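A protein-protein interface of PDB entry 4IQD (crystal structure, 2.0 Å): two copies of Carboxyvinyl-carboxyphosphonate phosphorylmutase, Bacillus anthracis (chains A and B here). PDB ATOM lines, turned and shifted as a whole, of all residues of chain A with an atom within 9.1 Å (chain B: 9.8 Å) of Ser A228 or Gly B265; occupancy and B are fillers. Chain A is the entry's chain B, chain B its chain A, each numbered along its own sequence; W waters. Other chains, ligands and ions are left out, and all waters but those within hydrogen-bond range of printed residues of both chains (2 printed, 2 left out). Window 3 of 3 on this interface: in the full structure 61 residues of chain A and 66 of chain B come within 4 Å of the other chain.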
ATOM      1  N   ILE A  30       5.521 -23.492  13.834  1.00  0.00           N
ATOM      2  CA  ILE A  30       5.002 -22.156  13.559  1.00  0.00           C
ATOM      3  C   ILE A  30       6.112 -21.223  13.067  1.00  0.00           C
ATOM      4  O   ILE A  30       7.241 -21.250  13.563  1.00  0.00           O
ATOM      5  CB  ILE A  30       4.252 -21.556  14.783  1.00  0.00           C
ATOM      6  CG1 ILE A  30       3.549 -20.246  14.406  1.00  0.00           C
ATOM      7  CG2 ILE A  30       5.192 -21.359  15.957  1.00  0.00           C
ATOM      8  CD1 ILE A  30       2.734 -19.629  15.532  1.00  0.00           C
ATOM      9  N   GLN A  32       7.917 -17.805  12.612  1.00  0.00           N
ATOM     10  CA  GLN A  32       8.095 -16.486  13.203  1.00  0.00           C
ATOM     11  C   GLN A  32       8.539 -15.484  12.152  1.00  0.00           C
ATOM     12  O   GLN A  32       9.507 -15.716  11.427  1.00  0.00           O
ATOM     13  CB  GLN A  32       9.106 -16.541  14.349  1.00  0.00           C
ATOM     14  CG  GLN A  32       8.527 -17.085  15.645  1.00  0.00           C
ATOM     15  CD  GLN A  32       9.540 -17.133  16.772  1.00  0.00           C
ATOM     16  OE1 GLN A  32      10.528 -17.855  16.701  1.00  0.00           O
ATOM     17  NE2 GLN A  32       9.289 -16.364  17.824  1.00  0.00           N
ATOM     18  N   PHE A  50      16.083 -16.187  11.812  1.00  0.00           N
ATOM     19  CA  PHE A  50      14.721 -16.134  11.297  1.00  0.00           C
ATOM     20  C   PHE A  50      14.694 -16.484   9.816  1.00  0.00           C
ATOM     21  O   PHE A  50      15.659 -16.236   9.092  1.00  0.00           O
ATOM     22  CB  PHE A  50      14.086 -14.773  11.572  1.00  0.00           C
ATOM     23  CG  PHE A  50      13.862 -14.506  13.030  1.00  0.00           C
ATOM     24  CD1 PHE A  50      12.728 -14.982  13.669  1.00  0.00           C
ATOM     25  CD2 PHE A  50      14.791 -13.799  13.769  1.00  0.00           C
ATOM     26  CE1 PHE A  50      12.525 -14.745  15.019  1.00  0.00           C
ATOM     27  CE2 PHE A  50      14.595 -13.562  15.117  1.00  0.00           C
ATOM     28  CZ  PHE A  50      13.459 -14.033  15.744  1.00  0.00           C
ATOM     29  N   PHE A 203     -10.192 -17.454  19.064  1.00  0.00           N
ATOM     30  CA  PHE A 203      -9.160 -17.968  18.168  1.00  0.00           C
ATOM     31  C   PHE A 203      -9.618 -19.297  17.593  1.00  0.00           C
ATOM     32  O   PHE A 203      -9.726 -19.463  16.380  1.00  0.00           O
ATOM     33  CB  PHE A 203      -7.836 -18.184  18.905  1.00  0.00           C
ATOM     34  CG  PHE A 203      -7.198 -16.926  19.408  1.00  0.00           C
ATOM     35  CD1 PHE A 203      -7.606 -15.685  18.950  1.00  0.00           C
ATOM     36  CD2 PHE A 203      -6.174 -16.988  20.337  1.00  0.00           C
ATOM     37  CE1 PHE A 203      -7.015 -14.530  19.417  1.00  0.00           C
ATOM     38  CE2 PHE A 203      -5.578 -15.838  20.809  1.00  0.00           C
ATOM     39  CZ  PHE A 203      -6.001 -14.606  20.348  1.00  0.00           C
ATOM     40  N   ALA A 216      -0.994 -14.415  13.273  1.00  0.00           N
ATOM     41  CA  ALA A 216      -1.174 -13.708  14.533  1.00  0.00           C
ATOM     42  C   ALA A 216      -0.323 -12.443  14.579  1.00  0.00           C
ATOM     43  O   ALA A 216       0.863 -12.469  14.259  1.00  0.00           O
ATOM     44  CB  ALA A 216      -0.821 -14.618  15.688  1.00  0.00           C
ATOM     45  N   MET A 218       1.565 -10.089  16.715  1.00  0.00           N
ATOM     46  CA  MET A 218       2.147  -9.871  18.031  1.00  0.00           C
ATOM     47  C   MET A 218       2.800  -8.493  18.138  1.00  0.00           C
ATOM     48  O   MET A 218       4.007  -8.384  18.343  1.00  0.00           O
ATOM     49  CB  MET A 218       3.149 -10.980  18.371  1.00  0.00           C
ATOM     50  CG  MET A 218       3.479 -11.115  19.857  1.00  0.00           C
ATOM     51  SD  MET A 218       1.914 -11.230  21.014  1.00  0.00           S
ATOM     52  CE  MET A 218       1.754  -9.349  21.511  1.00  0.00           C
ATOM     53  N   THR A 224      -3.705  -7.335  21.995  1.00  0.00           N
ATOM     54  CA  THR A 224      -3.302  -8.732  22.022  1.00  0.00           C
ATOM     55  C   THR A 224      -2.253  -9.007  23.101  1.00  0.00           C
ATOM     56  O   THR A 224      -1.226  -8.333  23.159  1.00  0.00           O
ATOM     57  CB  THR A 224      -2.772  -9.171  20.644  1.00  0.00           C
ATOM     58  OG1 THR A 224      -3.801  -8.993  19.663  1.00  0.00           O
ATOM     59  CG2 THR A 224      -2.345 -10.628  20.663  1.00  0.00           C
ATOM     60  N   PRO A 225      -2.524  -9.999  23.967  1.00  0.00           N
ATOM     61  CA  PRO A 225      -1.615 -10.421  25.039  1.00  0.00           C
ATOM     62  C   PRO A 225      -0.305 -10.964  24.486  1.00  0.00           C
ATOM     63  O   PRO A 225      -0.239 -11.317  23.311  1.00  0.00           O
ATOM     64  CB  PRO A 225      -2.387 -11.549  25.728  1.00  0.00           C
ATOM     65  CG  PRO A 225      -3.804 -11.314  25.381  1.00  0.00           C
ATOM     66  CD  PRO A 225      -3.795 -10.740  24.006  1.00  0.00           C
ATOM     67  N   TYR A 226       0.715 -11.051  25.334  1.00  0.00           N
ATOM     68  CA  TYR A 226       2.047 -11.441  24.890  1.00  0.00           C
ATOM     69  C   TYR A 226       2.259 -12.954  24.890  1.00  0.00           C
ATOM     70  O   TYR A 226       3.134 -13.473  25.582  1.00  0.00           O
ATOM     71  CB  TYR A 226       3.116 -10.721  25.717  1.00  0.00           C
ATOM     72  CG  TYR A 226       3.042  -9.218  25.577  1.00  0.00           C
ATOM     73  CD1 TYR A 226       2.407  -8.442  26.537  1.00  0.00           C
ATOM     74  CD2 TYR A 226       3.587  -8.577  24.469  1.00  0.00           C
ATOM     75  CE1 TYR A 226       2.328  -7.068  26.407  1.00  0.00           C
ATOM     76  CE2 TYR A 226       3.514  -7.204  24.328  1.00  0.00           C
ATOM     77  CZ  TYR A 226       2.883  -6.453  25.299  1.00  0.00           C
ATOM     78  OH  TYR A 226       2.807  -5.085  25.161  1.00  0.00           O
ATOM     79  N   TYR A 227       1.447 -13.644  24.094  1.00  0.00           N
ATOM     80  CA  TYR A 227       1.558 -15.084  23.908  1.00  0.00           C
ATOM     81  C   TYR A 227       2.878 -15.442  23.240  1.00  0.00           C
ATOM     82  O   TYR A 227       3.371 -14.704  22.390  1.00  0.00           O
ATOM     83  CB  TYR A 227       0.420 -15.598  23.024  1.00  0.00           C
ATOM     84  CG  TYR A 227      -0.960 -15.541  23.636  1.00  0.00           C
ATOM     85  CD1 TYR A 227      -1.934 -14.698  23.116  1.00  0.00           C
ATOM     86  CD2 TYR A 227      -1.298 -16.340  24.716  1.00  0.00           C
ATOM     87  CE1 TYR A 227      -3.200 -14.646  23.659  1.00  0.00           C
ATOM     88  CE2 TYR A 227      -2.563 -16.294  25.268  1.00  0.00           C
ATOM     89  CZ  TYR A 227      -3.510 -15.446  24.734  1.00  0.00           C
ATOM     90  OH  TYR A 227      -4.773 -15.392  25.275  1.00  0.00           O
ATOM     91  N   SER A 228       3.439 -16.584  23.616  1.00  0.00           N
ATOM     92  CA  SER A 228       4.632 -17.087  22.954  1.00  0.00           C
ATOM     93  C   SER A 228       4.245 -17.685  21.608  1.00  0.00           C
ATOM     94  O   SER A 228       3.072 -17.964  21.360  1.00  0.00           O
ATOM     95  CB  SER A 228       5.335 -18.134  23.819  1.00  0.00           C
ATOM     96  OG  SER A 228       4.595 -19.340  23.869  1.00  0.00           O
ATOM     97  N   ALA A 229       5.233 -17.871  20.741  1.00  0.00           N
ATOM     98  CA  ALA A 229       4.983 -18.410  19.412  1.00  0.00           C
ATOM     99  C   ALA A 229       4.351 -19.789  19.505  1.00  0.00           C
ATOM    100  O   ALA A 229       3.469 -20.138  18.724  1.00  0.00           O
ATOM    101  CB  ALA A 229       6.276 -18.478  18.626  1.00  0.00           C
ATOM    102  N   GLU A 230       4.804 -20.564  20.483  1.00  0.00           N
ATOM    103  CA  GLU A 230       4.340 -21.928  20.649  1.00  0.00           C
ATOM    104  C   GLU A 230       2.889 -21.961  21.103  1.00  0.00           C
ATOM    105  O   GLU A 230       2.149 -22.877  20.760  1.00  0.00           O
ATOM    106  CB  GLU A 230       5.228 -22.676  21.640  1.00  0.00           C
ATOM    107  CG  GLU A 230       5.319 -24.162  21.360  1.00  0.00           C
ATOM    108  CD  GLU A 230       5.703 -24.454  19.922  1.00  0.00           C
ATOM    109  OE1 GLU A 230       6.633 -23.798  19.406  1.00  0.00           O
ATOM    110  OE2 GLU A 230       5.066 -25.332  19.304  1.00  0.00           O
ATOM    111  N   GLU A 231       2.488 -20.954  21.873  1.00  0.00           N
ATOM    112  CA  GLU A 231       1.115 -20.854  22.355  1.00  0.00           C
ATOM    113  C   GLU A 231       0.169 -20.530  21.211  1.00  0.00           C
ATOM    114  O   GLU A 231      -0.903 -21.115  21.102  1.00  0.00           O
ATOM    115  CB  GLU A 231       1.006 -19.806  23.459  1.00  0.00           C
ATOM    116  CG  GLU A 231       1.648 -20.242  24.765  1.00  0.00           C
ATOM    117  CD  GLU A 231       1.604 -19.168  25.833  1.00  0.00           C
ATOM    118  OE1 GLU A 231       1.746 -17.978  25.490  1.00  0.00           O
ATOM    119  OE2 GLU A 231       1.428 -19.514  27.020  1.00  0.00           O
ATOM    120  N   PHE A 232       0.582 -19.603  20.354  1.00  0.00           N
ATOM    121  CA  PHE A 232      -0.154 -19.294  19.138  1.00  0.00           C
ATOM    122  C   PHE A 232      -0.369 -20.545  18.298  1.00  0.00           C
ATOM    123  O   PHE A 232      -1.441 -20.750  17.735  1.00  0.00           O
ATOM    124  CB  PHE A 232       0.604 -18.253  18.320  1.00  0.00           C
ATOM    125  CG  PHE A 232       0.408 -16.848  18.800  1.00  0.00           C
ATOM    126  CD1 PHE A 232       1.493 -16.019  19.014  1.00  0.00           C
ATOM    127  CD2 PHE A 232      -0.864 -16.356  19.028  1.00  0.00           C
ATOM    128  CE1 PHE A 232       1.317 -14.728  19.454  1.00  0.00           C
ATOM    129  CE2 PHE A 232      -1.048 -15.063  19.466  1.00  0.00           C
ATOM    130  CZ  PHE A 232       0.046 -14.247  19.679  1.00  0.00           C
ATOM    131  N   ALA A 233       0.661 -21.378  18.223  1.00  0.00           N
ATOM    132  CA  ALA A 233       0.593 -22.615  17.462  1.00  0.00           C
ATOM    133  C   ALA A 233      -0.460 -23.540  18.057  1.00  0.00           C
ATOM    134  O   ALA A 233      -1.268 -24.125  17.336  1.00  0.00           O
ATOM    135  CB  ALA A 233       1.951 -23.297  17.441  1.00  0.00           C
ATOM    136  N   ASN A 234      -0.448 -23.655  19.382  1.00  0.00           N
ATOM    137  CA  ASN A 234      -1.420 -24.477  20.093  1.00  0.00           C
ATOM    138  C   ASN A 234      -2.836 -23.927  19.974  1.00  0.00           C
ATOM    139  O   ASN A 234      -3.810 -24.651  20.179  1.00  0.00           O
ATOM    140  CB  ASN A 234      -1.037 -24.605  21.571  1.00  0.00           C
ATOM    141  CG  ASN A 234       0.265 -25.356  21.778  1.00  0.00           C
ATOM    142  OD1 ASN A 234       1.074 -25.489  20.861  1.00  0.00           O
ATOM    143  ND2 ASN A 234       0.474 -25.854  22.991  1.00  0.00           N
ATOM    144  N   MET A 235      -2.947 -22.645  19.644  1.00  0.00           N
ATOM    145  CA  MET A 235      -4.251 -21.996  19.567  1.00  0.00           C
ATOM    146  C   MET A 235      -4.805 -21.919  18.143  1.00  0.00           C
ATOM    147  O   MET A 235      -5.907 -21.417  17.922  1.00  0.00           O
ATOM    148  CB  MET A 235      -4.216 -20.621  20.244  1.00  0.00           C
ATOM    149  CG  MET A 235      -4.013 -20.720  21.753  1.00  0.00           C
ATOM    150  SD  MET A 235      -4.060 -19.038  22.754  1.00  0.00           S
ATOM    151  CE  MET A 235      -3.105 -19.624  24.351  1.00  0.00           C
ATOM    152  N   PHE A 237      -2.758 -21.016  15.189  1.00  0.00           N
ATOM    153  CA  PHE A 237      -1.997 -20.192  14.253  1.00  0.00           C
ATOM    154  C   PHE A 237      -0.821 -20.922  13.621  1.00  0.00           C
ATOM    155  O   PHE A 237      -0.214 -21.798  14.235  1.00  0.00           O
ATOM    156  CB  PHE A 237      -1.515 -18.911  14.932  1.00  0.00           C
ATOM    157  CG  PHE A 237      -2.627 -18.015  15.381  1.00  0.00           C
ATOM    158  CD1 PHE A 237      -3.143 -17.054  14.531  1.00  0.00           C
ATOM    159  CD2 PHE A 237      -3.164 -18.142  16.648  1.00  0.00           C
ATOM    160  CE1 PHE A 237      -4.169 -16.228  14.939  1.00  0.00           C
ATOM    161  CE2 PHE A 237      -4.188 -17.323  17.061  1.00  0.00           C
ATOM    162  CZ  PHE A 237      -4.693 -16.364  16.205  1.00  0.00           C
ATOM    163  N   MET A 239       1.537 -18.942  11.862  1.00  0.00           N
ATOM    164  CA  MET A 239       2.574 -17.920  11.772  1.00  0.00           C
ATOM    165  C   MET A 239       2.224 -16.716  12.631  1.00  0.00           C
ATOM    166  O   MET A 239       1.056 -16.467  12.926  1.00  0.00           O
ATOM    167  CB  MET A 239       2.769 -17.469  10.332  1.00  0.00           C
ATOM    168  CG  MET A 239       1.495 -16.988   9.688  1.00  0.00           C
ATOM    169  SD  MET A 239       1.813 -16.309   7.908  1.00  0.00           S
ATOM    170  CE  MET A 239      -0.026 -16.284   7.276  1.00  0.00           C
ATOM    171  N   VAL A 240       3.246 -15.966  13.025  1.00  0.00           N
ATOM    172  CA  VAL A 240       3.053 -14.805  13.877  1.00  0.00           C
ATOM    173  C   VAL A 240       4.035 -13.708  13.497  1.00  0.00           C
ATOM    174  O   VAL A 240       5.221 -13.966  13.306  1.00  0.00           O
ATOM    175  CB  VAL A 240       3.212 -15.176  15.366  1.00  0.00           C
ATOM    176  CG1 VAL A 240       4.477 -15.986  15.584  1.00  0.00           C
ATOM    177  CG2 VAL A 240       3.201 -13.932  16.240  1.00  0.00           C
ATOM    178  N   ILE A 241       3.540 -12.484  13.363  1.00  0.00           N
ATOM    179  CA  ILE A 241       4.411 -11.369  13.020  1.00  0.00           C
ATOM    180  C   ILE A 241       4.801 -10.536  14.233  1.00  0.00           C
ATOM    181  O   ILE A 241       4.114 -10.532  15.252  1.00  0.00           O
ATOM    182  CB  ILE A 241       3.795 -10.448  11.947  1.00  0.00           C
ATOM    183  CG1 ILE A 241       2.441  -9.911  12.406  1.00  0.00           C
ATOM    184  CG2 ILE A 241       3.655 -11.181  10.629  1.00  0.00           C
ATOM    185  CD1 ILE A 241       1.779  -9.013  11.382  1.00  0.00           C
ATOM    186  N   TYR A 242       5.927  -9.848  14.106  1.00  0.00           N
ATOM    187  CA  TYR A 242       6.397  -8.907  15.110  1.00  0.00           C
ATOM    188  C   TYR A 242       6.753  -7.633  14.357  1.00  0.00           C
ATOM    189  O   TYR A 242       7.923  -7.340  14.140  1.00  0.00           O
ATOM    190  CB  TYR A 242       7.610  -9.476  15.846  1.00  0.00           C
ATOM    191  CG  TYR A 242       7.346 -10.832  16.465  1.00  0.00           C
ATOM    192  CD1 TYR A 242       6.827 -10.941  17.750  1.00  0.00           C
ATOM    193  CD2 TYR A 242       7.602 -12.004  15.760  1.00  0.00           C
ATOM    194  CE1 TYR A 242       6.574 -12.177  18.319  1.00  0.00           C
ATOM    195  CE2 TYR A 242       7.352 -13.241  16.317  1.00  0.00           C
ATOM    196  CZ  TYR A 242       6.839 -13.324  17.597  1.00  0.00           C
ATOM    197  OH  TYR A 242       6.591 -14.557  18.156  1.00  0.00           O
ATOM    198  N   VAL B 257      16.825  -8.005  20.717  1.00  0.00           N
ATOM    199  CA  VAL B 257      15.397  -8.269  20.724  1.00  0.00           C
ATOM    200  C   VAL B 257      15.052  -9.439  19.805  1.00  0.00           C
ATOM    201  O   VAL B 257      14.118 -10.192  20.070  1.00  0.00           O
ATOM    202  CB  VAL B 257      14.569  -7.005  20.386  1.00  0.00           C
ATOM    203  CG1 VAL B 257      14.663  -6.664  18.910  1.00  0.00           C
ATOM    204  CG2 VAL B 257      13.122  -7.190  20.802  1.00  0.00           C
ATOM    205  N   PHE B 258      15.828  -9.605  18.739  1.00  0.00           N
ATOM    206  CA  PHE B 258      15.645 -10.732  17.833  1.00  0.00           C
ATOM    207  C   PHE B 258      16.087 -12.022  18.498  1.00  0.00           C
ATOM    208  O   PHE B 258      15.429 -13.055  18.371  1.00  0.00           O
ATOM    209  CB  PHE B 258      16.445 -10.520  16.553  1.00  0.00           C
ATOM    210  CG  PHE B 258      15.897  -9.445  15.673  1.00  0.00           C
ATOM    211  CD1 PHE B 258      14.572  -9.063  15.771  1.00  0.00           C
ATOM    212  CD2 PHE B 258      16.702  -8.819  14.741  1.00  0.00           C
ATOM    213  CE1 PHE B 258      14.061  -8.075  14.959  1.00  0.00           C
ATOM    214  CE2 PHE B 258      16.196  -7.828  13.923  1.00  0.00           C
ATOM    215  CZ  PHE B 258      14.872  -7.456  14.034  1.00  0.00           C
ATOM    216  N   THR B 259      17.216 -11.953  19.194  1.00  0.00           N
ATOM    217  CA  THR B 259      17.701 -13.071  19.983  1.00  0.00           C
ATOM    218  C   THR B 259      16.611 -13.506  20.948  1.00  0.00           C
ATOM    219  O   THR B 259      16.318 -14.691  21.082  1.00  0.00           O
ATOM    220  CB  THR B 259      18.953 -12.677  20.785  1.00  0.00           C
ATOM    221  OG1 THR B 259      19.976 -12.229  19.889  1.00  0.00           O
ATOM    222  CG2 THR B 259      19.474 -13.850  21.585  1.00  0.00           C
ATOM    223  N   LEU B 260      15.999 -12.521  21.596  1.00  0.00           N
ATOM    224  CA  LEU B 260      14.972 -12.760  22.596  1.00  0.00           C
ATOM    225  C   LEU B 260      13.751 -13.451  22.006  1.00  0.00           C
ATOM    226  O   LEU B 260      13.258 -14.429  22.566  1.00  0.00           O
ATOM    227  CB  LEU B 260      14.561 -11.438  23.240  1.00  0.00           C
ATOM    228  CG  LEU B 260      13.649 -11.502  24.462  1.00  0.00           C
ATOM    229  CD1 LEU B 260      14.284 -12.319  25.574  1.00  0.00           C
ATOM    230  CD2 LEU B 260      13.358 -10.095  24.939  1.00  0.00           C
ATOM    231  N   ILE B 261      13.266 -12.944  20.877  1.00  0.00           N
ATOM    232  CA  ILE B 261      12.090 -13.520  20.235  1.00  0.00           C
ATOM    233  C   ILE B 261      12.366 -14.935  19.737  1.00  0.00           C
ATOM    234  O   ILE B 261      11.492 -15.797  19.783  1.00  0.00           O
ATOM    235  CB  ILE B 261      11.585 -12.650  19.061  1.00  0.00           C
ATOM    236  CG1 ILE B 261      11.239 -11.239  19.541  1.00  0.00           C
ATOM    237  CG2 ILE B 261      10.367 -13.278  18.413  1.00  0.00           C
ATOM    238  CD1 ILE B 261      10.742 -10.327  18.443  1.00  0.00           C
ATOM    239  N   LYS B 262      13.581 -15.179  19.266  1.00  0.00           N
ATOM    240  CA  LYS B 262      13.930 -16.510  18.788  1.00  0.00           C
ATOM    241  C   LYS B 262      14.108 -17.470  19.955  1.00  0.00           C
ATOM    242  O   LYS B 262      13.654 -18.610  19.906  1.00  0.00           O
ATOM    243  CB  LYS B 262      15.196 -16.481  17.927  1.00  0.00           C
ATOM    244  CG  LYS B 262      15.471 -17.789  17.185  1.00  0.00           C
ATOM    245  CD  LYS B 262      14.176 -18.422  16.688  1.00  0.00           C
ATOM    246  CE  LYS B 262      14.418 -19.534  15.677  1.00  0.00           C
ATOM    247  NZ  LYS B 262      14.407 -19.017  14.281  1.00  0.00           N
ATOM    248  N   GLU B 263      14.770 -16.996  21.004  1.00  0.00           N
ATOM    249  CA  GLU B 263      15.055 -17.822  22.166  1.00  0.00           C
ATOM    250  C   GLU B 263      13.817 -18.121  22.993  1.00  0.00           C
ATOM    251  O   GLU B 263      13.535 -19.274  23.310  1.00  0.00           O
ATOM    252  CB  GLU B 263      16.084 -17.143  23.065  1.00  0.00           C
ATOM    253  CG  GLU B 263      17.516 -17.275  22.603  1.00  0.00           C
ATOM    254  CD  GLU B 263      18.491 -17.058  23.739  1.00  0.00           C
ATOM    255  OE1 GLU B 263      18.031 -16.934  24.893  1.00  0.00           O
ATOM    256  OE2 GLU B 263      19.713 -17.013  23.483  1.00  0.00           O
ATOM    257  N   THR B 264      13.092 -17.070  23.354  1.00  0.00           N
ATOM    258  CA  THR B 264      11.990 -17.195  24.296  1.00  0.00           C
ATOM    259  C   THR B 264      10.636 -17.303  23.608  1.00  0.00           C
ATOM    260  O   THR B 264       9.644 -17.659  24.239  1.00  0.00           O
ATOM    261  CB  THR B 264      11.959 -16.006  25.262  1.00  0.00           C
ATOM    262  OG1 THR B 264      11.548 -14.829  24.557  1.00  0.00           O
ATOM    263  CG2 THR B 264      13.338 -15.782  25.857  1.00  0.00           C
ATOM    264  N   GLY B 265      10.595 -16.992  22.317  1.00  0.00           N
ATOM    265  CA  GLY B 265       9.355 -17.052  21.565  1.00  0.00           C
ATOM    266  C   GLY B 265       8.504 -15.804  21.713  1.00  0.00           C
ATOM    267  O   GLY B 265       7.432 -15.705  21.117  1.00  0.00           O
ATOM    268  N   SER B 266       8.988 -14.846  22.500  1.00  0.00           N
ATOM    269  CA  SER B 266       8.231 -13.630  22.789  1.00  0.00           C
ATOM    270  C   SER B 266       9.156 -12.435  23.020  1.00  0.00           C
ATOM    271  O   SER B 266      10.317 -12.604  23.391  1.00  0.00           O
ATOM    272  CB  SER B 266       7.342 -13.854  24.016  1.00  0.00           C
ATOM    273  OG  SER B 266       6.586 -12.698  24.326  1.00  0.00           O
ATOM    274  N   GLN B 267       8.644 -11.230  22.791  1.00  0.00           N
ATOM    275  CA  GLN B 267       9.428 -10.028  23.041  1.00  0.00           C
ATOM    276  C   GLN B 267       9.091  -9.455  24.412  1.00  0.00           C
ATOM    277  O   GLN B 267       9.436  -8.317  24.720  1.00  0.00           O
ATOM    278  CB  GLN B 267       9.219  -8.982  21.941  1.00  0.00           C
ATOM    279  CG  GLN B 267       7.873  -8.278  21.966  1.00  0.00           C
ATOM    280  CD  GLN B 267       6.812  -8.997  21.159  1.00  0.00           C
ATOM    281  OE1 GLN B 267       6.604 -10.200  21.312  1.00  0.00           O
ATOM    282  NE2 GLN B 267       6.134  -8.258  20.292  1.00  0.00           N
ATOM    283  N   LYS B 268       8.418 -10.275  25.217  1.00  0.00           N
ATOM    284  CA  LYS B 268       8.031  -9.957  26.597  1.00  0.00           C
ATOM    285  C   LYS B 268       9.013  -9.134  27.424  1.00  0.00           C
ATOM    286  O   LYS B 268       8.642  -8.149  28.062  1.00  0.00           O
ATOM    287  CB  LYS B 268       7.830 -11.274  27.347  1.00  0.00           C
ATOM    288  CG  LYS B 268       6.413 -11.632  27.705  1.00  0.00           C
ATOM    289  CD  LYS B 268       6.371 -13.059  28.225  1.00  0.00           C
ATOM    290  CE  LYS B 268       5.324 -13.234  29.298  1.00  0.00           C
ATOM    291  NZ  LYS B 268       5.214 -14.651  29.740  1.00  0.00           N
ATOM    292  N   ASP B 269      10.269  -9.559  27.417  1.00  0.00           N
ATOM    293  CA  ASP B 269      11.245  -9.035  28.356  1.00  0.00           C
ATOM    294  C   ASP B 269      11.921  -7.755  27.875  1.00  0.00           C
ATOM    295  O   ASP B 269      12.701  -7.148  28.608  1.00  0.00           O
ATOM    296  CB  ASP B 269      12.291 -10.106  28.676  1.00  0.00           C
ATOM    297  CG  ASP B 269      11.671 -11.389  29.198  1.00  0.00           C
ATOM    298  OD1 ASP B 269      10.584 -11.323  29.816  1.00  0.00           O
ATOM    299  OD2 ASP B 269      12.269 -12.464  28.995  1.00  0.00           O
HETATM  300  O   HOH W   1       5.081 -15.697  26.643  1.00  0.00           O
HETATM  301  O   HOH W   2       5.082 -14.417  20.202  1.00  0.00           O
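The side-chain amide nitrogen of Gln B267 sits at hydrogen-bond distance from the backbone carbonyl oxygen of Met A218, at 2.9 Å.
O of Gly B265 is in hydrogen-bond range of N of Ala A229 (3.1 Å).
NE2 of Gln A32 is in hydrogen-bond range of O of Ile B261.
The side-chain hydroxyl (OH) of Tyr A242 sits at hydrogen-bond distance from the backbone carbonyl oxygen (O) of Gly B265, 3.3 Å away.
The backbone NH (N) of Ser A228 is in hydrogen-bond range of the side-chain carboxylate (OE1) of Glu A231 (2.9 Å).
The side-chain hydroxyl of Tyr A242 is in hydrogen-bond range of the side-chain amide nitrogen of Gln A32 (3.3 Å).
The backbone NH of Met A218 sits at hydrogen-bond distance from the backbone carbonyl oxygen of Ile A241 (3.0 Å).
The side-chain hydroxyl (OG) of Ser B266 is in hydrogen-bond range of the backbone NH (N) of Lys B268 (3.2 Å).
OG1 of Thr B264 lies within hydrogen-bond range of O of Ser B266, 2.8 Å away.
OE1 of Gln A32 touches CD of Lys B262, at 3.7 Å.
Gln A32 touches Gly B265 (NE2 to CA, 3.8 Å).
Phe B258 touches Phe A50 (O to CE2, 3.4 Å).
Lys B262 touches Phe A50.
O of Tyr A226 touches OG of Ser B266 (3.8 Å).
Lys B268 touches Tyr A226 (CG to CB, 3.96 Å).
CA of Ser A228 touches O of Gly B265, at 3.6 Å.
CZ of Tyr A242 touches CG2 of Ile B261, 3.6 Å away.
CE1 of Tyr A242 touches OE1 of Gln B267 (3.6 Å).
Of chain B, only Gly B265 comes within 4 Å of Ser A228.
No residue of chain B comes within 4 Å of Glu A231.
Val B257 touches none of the printed residues of chain A.
Printed residues of chain A within 4 Å of Phe B258: Phe A50 (3.4 Å).
Printed residues of chain A within 4 Å of Ile B261: Gln A32 (3.0 Å) and Tyr A242 (3.6 Å).
Of the printed residues of chain A, Lys B262 touches Gln A32 and Phe A50.
No residue of chain A comes within 4 Å of Thr B264.
Gly B265 touches four residues of chain A.
The nearest printed residue of chain B that does not touch Ser A228 is Ser B266 (4.4 Å).
The nearest residue of chain A that does not touch Gly B265 is Tyr A227 (4.4 Å).
The nearest printed residue of chain B that does not touch Met A218 is Ser B266 (5.7 Å).
Printed residues of chain B that touch a printed residue of chain A: Phe B258, Ile B261, Lys B262, Gly B265, Ser B266, Gln B267 and Lys B268.
Hydrophobic or aromatic side chains of chain B within 4 Å of the printed part of chain A: Phe B258 and Ile B261.
Of the 23 printed residues of chain A, 7 touch a printed residue of chain B.
Printed residues of chain A that touch a printed residue of chain B: Gln A32, Phe A50, Met A218, Tyr A226, Ser A228, Ala A229 and Tyr A242.
Along chain A the printed residues that touch a printed residue of chain B span positions 32 to 242.
Among the printed residues, no Asp or Glu carboxylate lies within 4 Å of a Lys or Arg side-chain nitrogen of the other chain.
No position is printed for both chains.
Water W2 lies within hydrogen-bond range of OH of Tyr A242 (2.5 Å), O of Tyr A227 (2.8 Å), O of Gly B265 (2.8 Å) and N of Ala A229 (3.5 Å).
Water W1 bridges the backbone carbonyl oxygen (O) of Tyr A226 (3.1 Å) and the side-chain amino group (NZ) of Lys B268 (3.3 Å).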
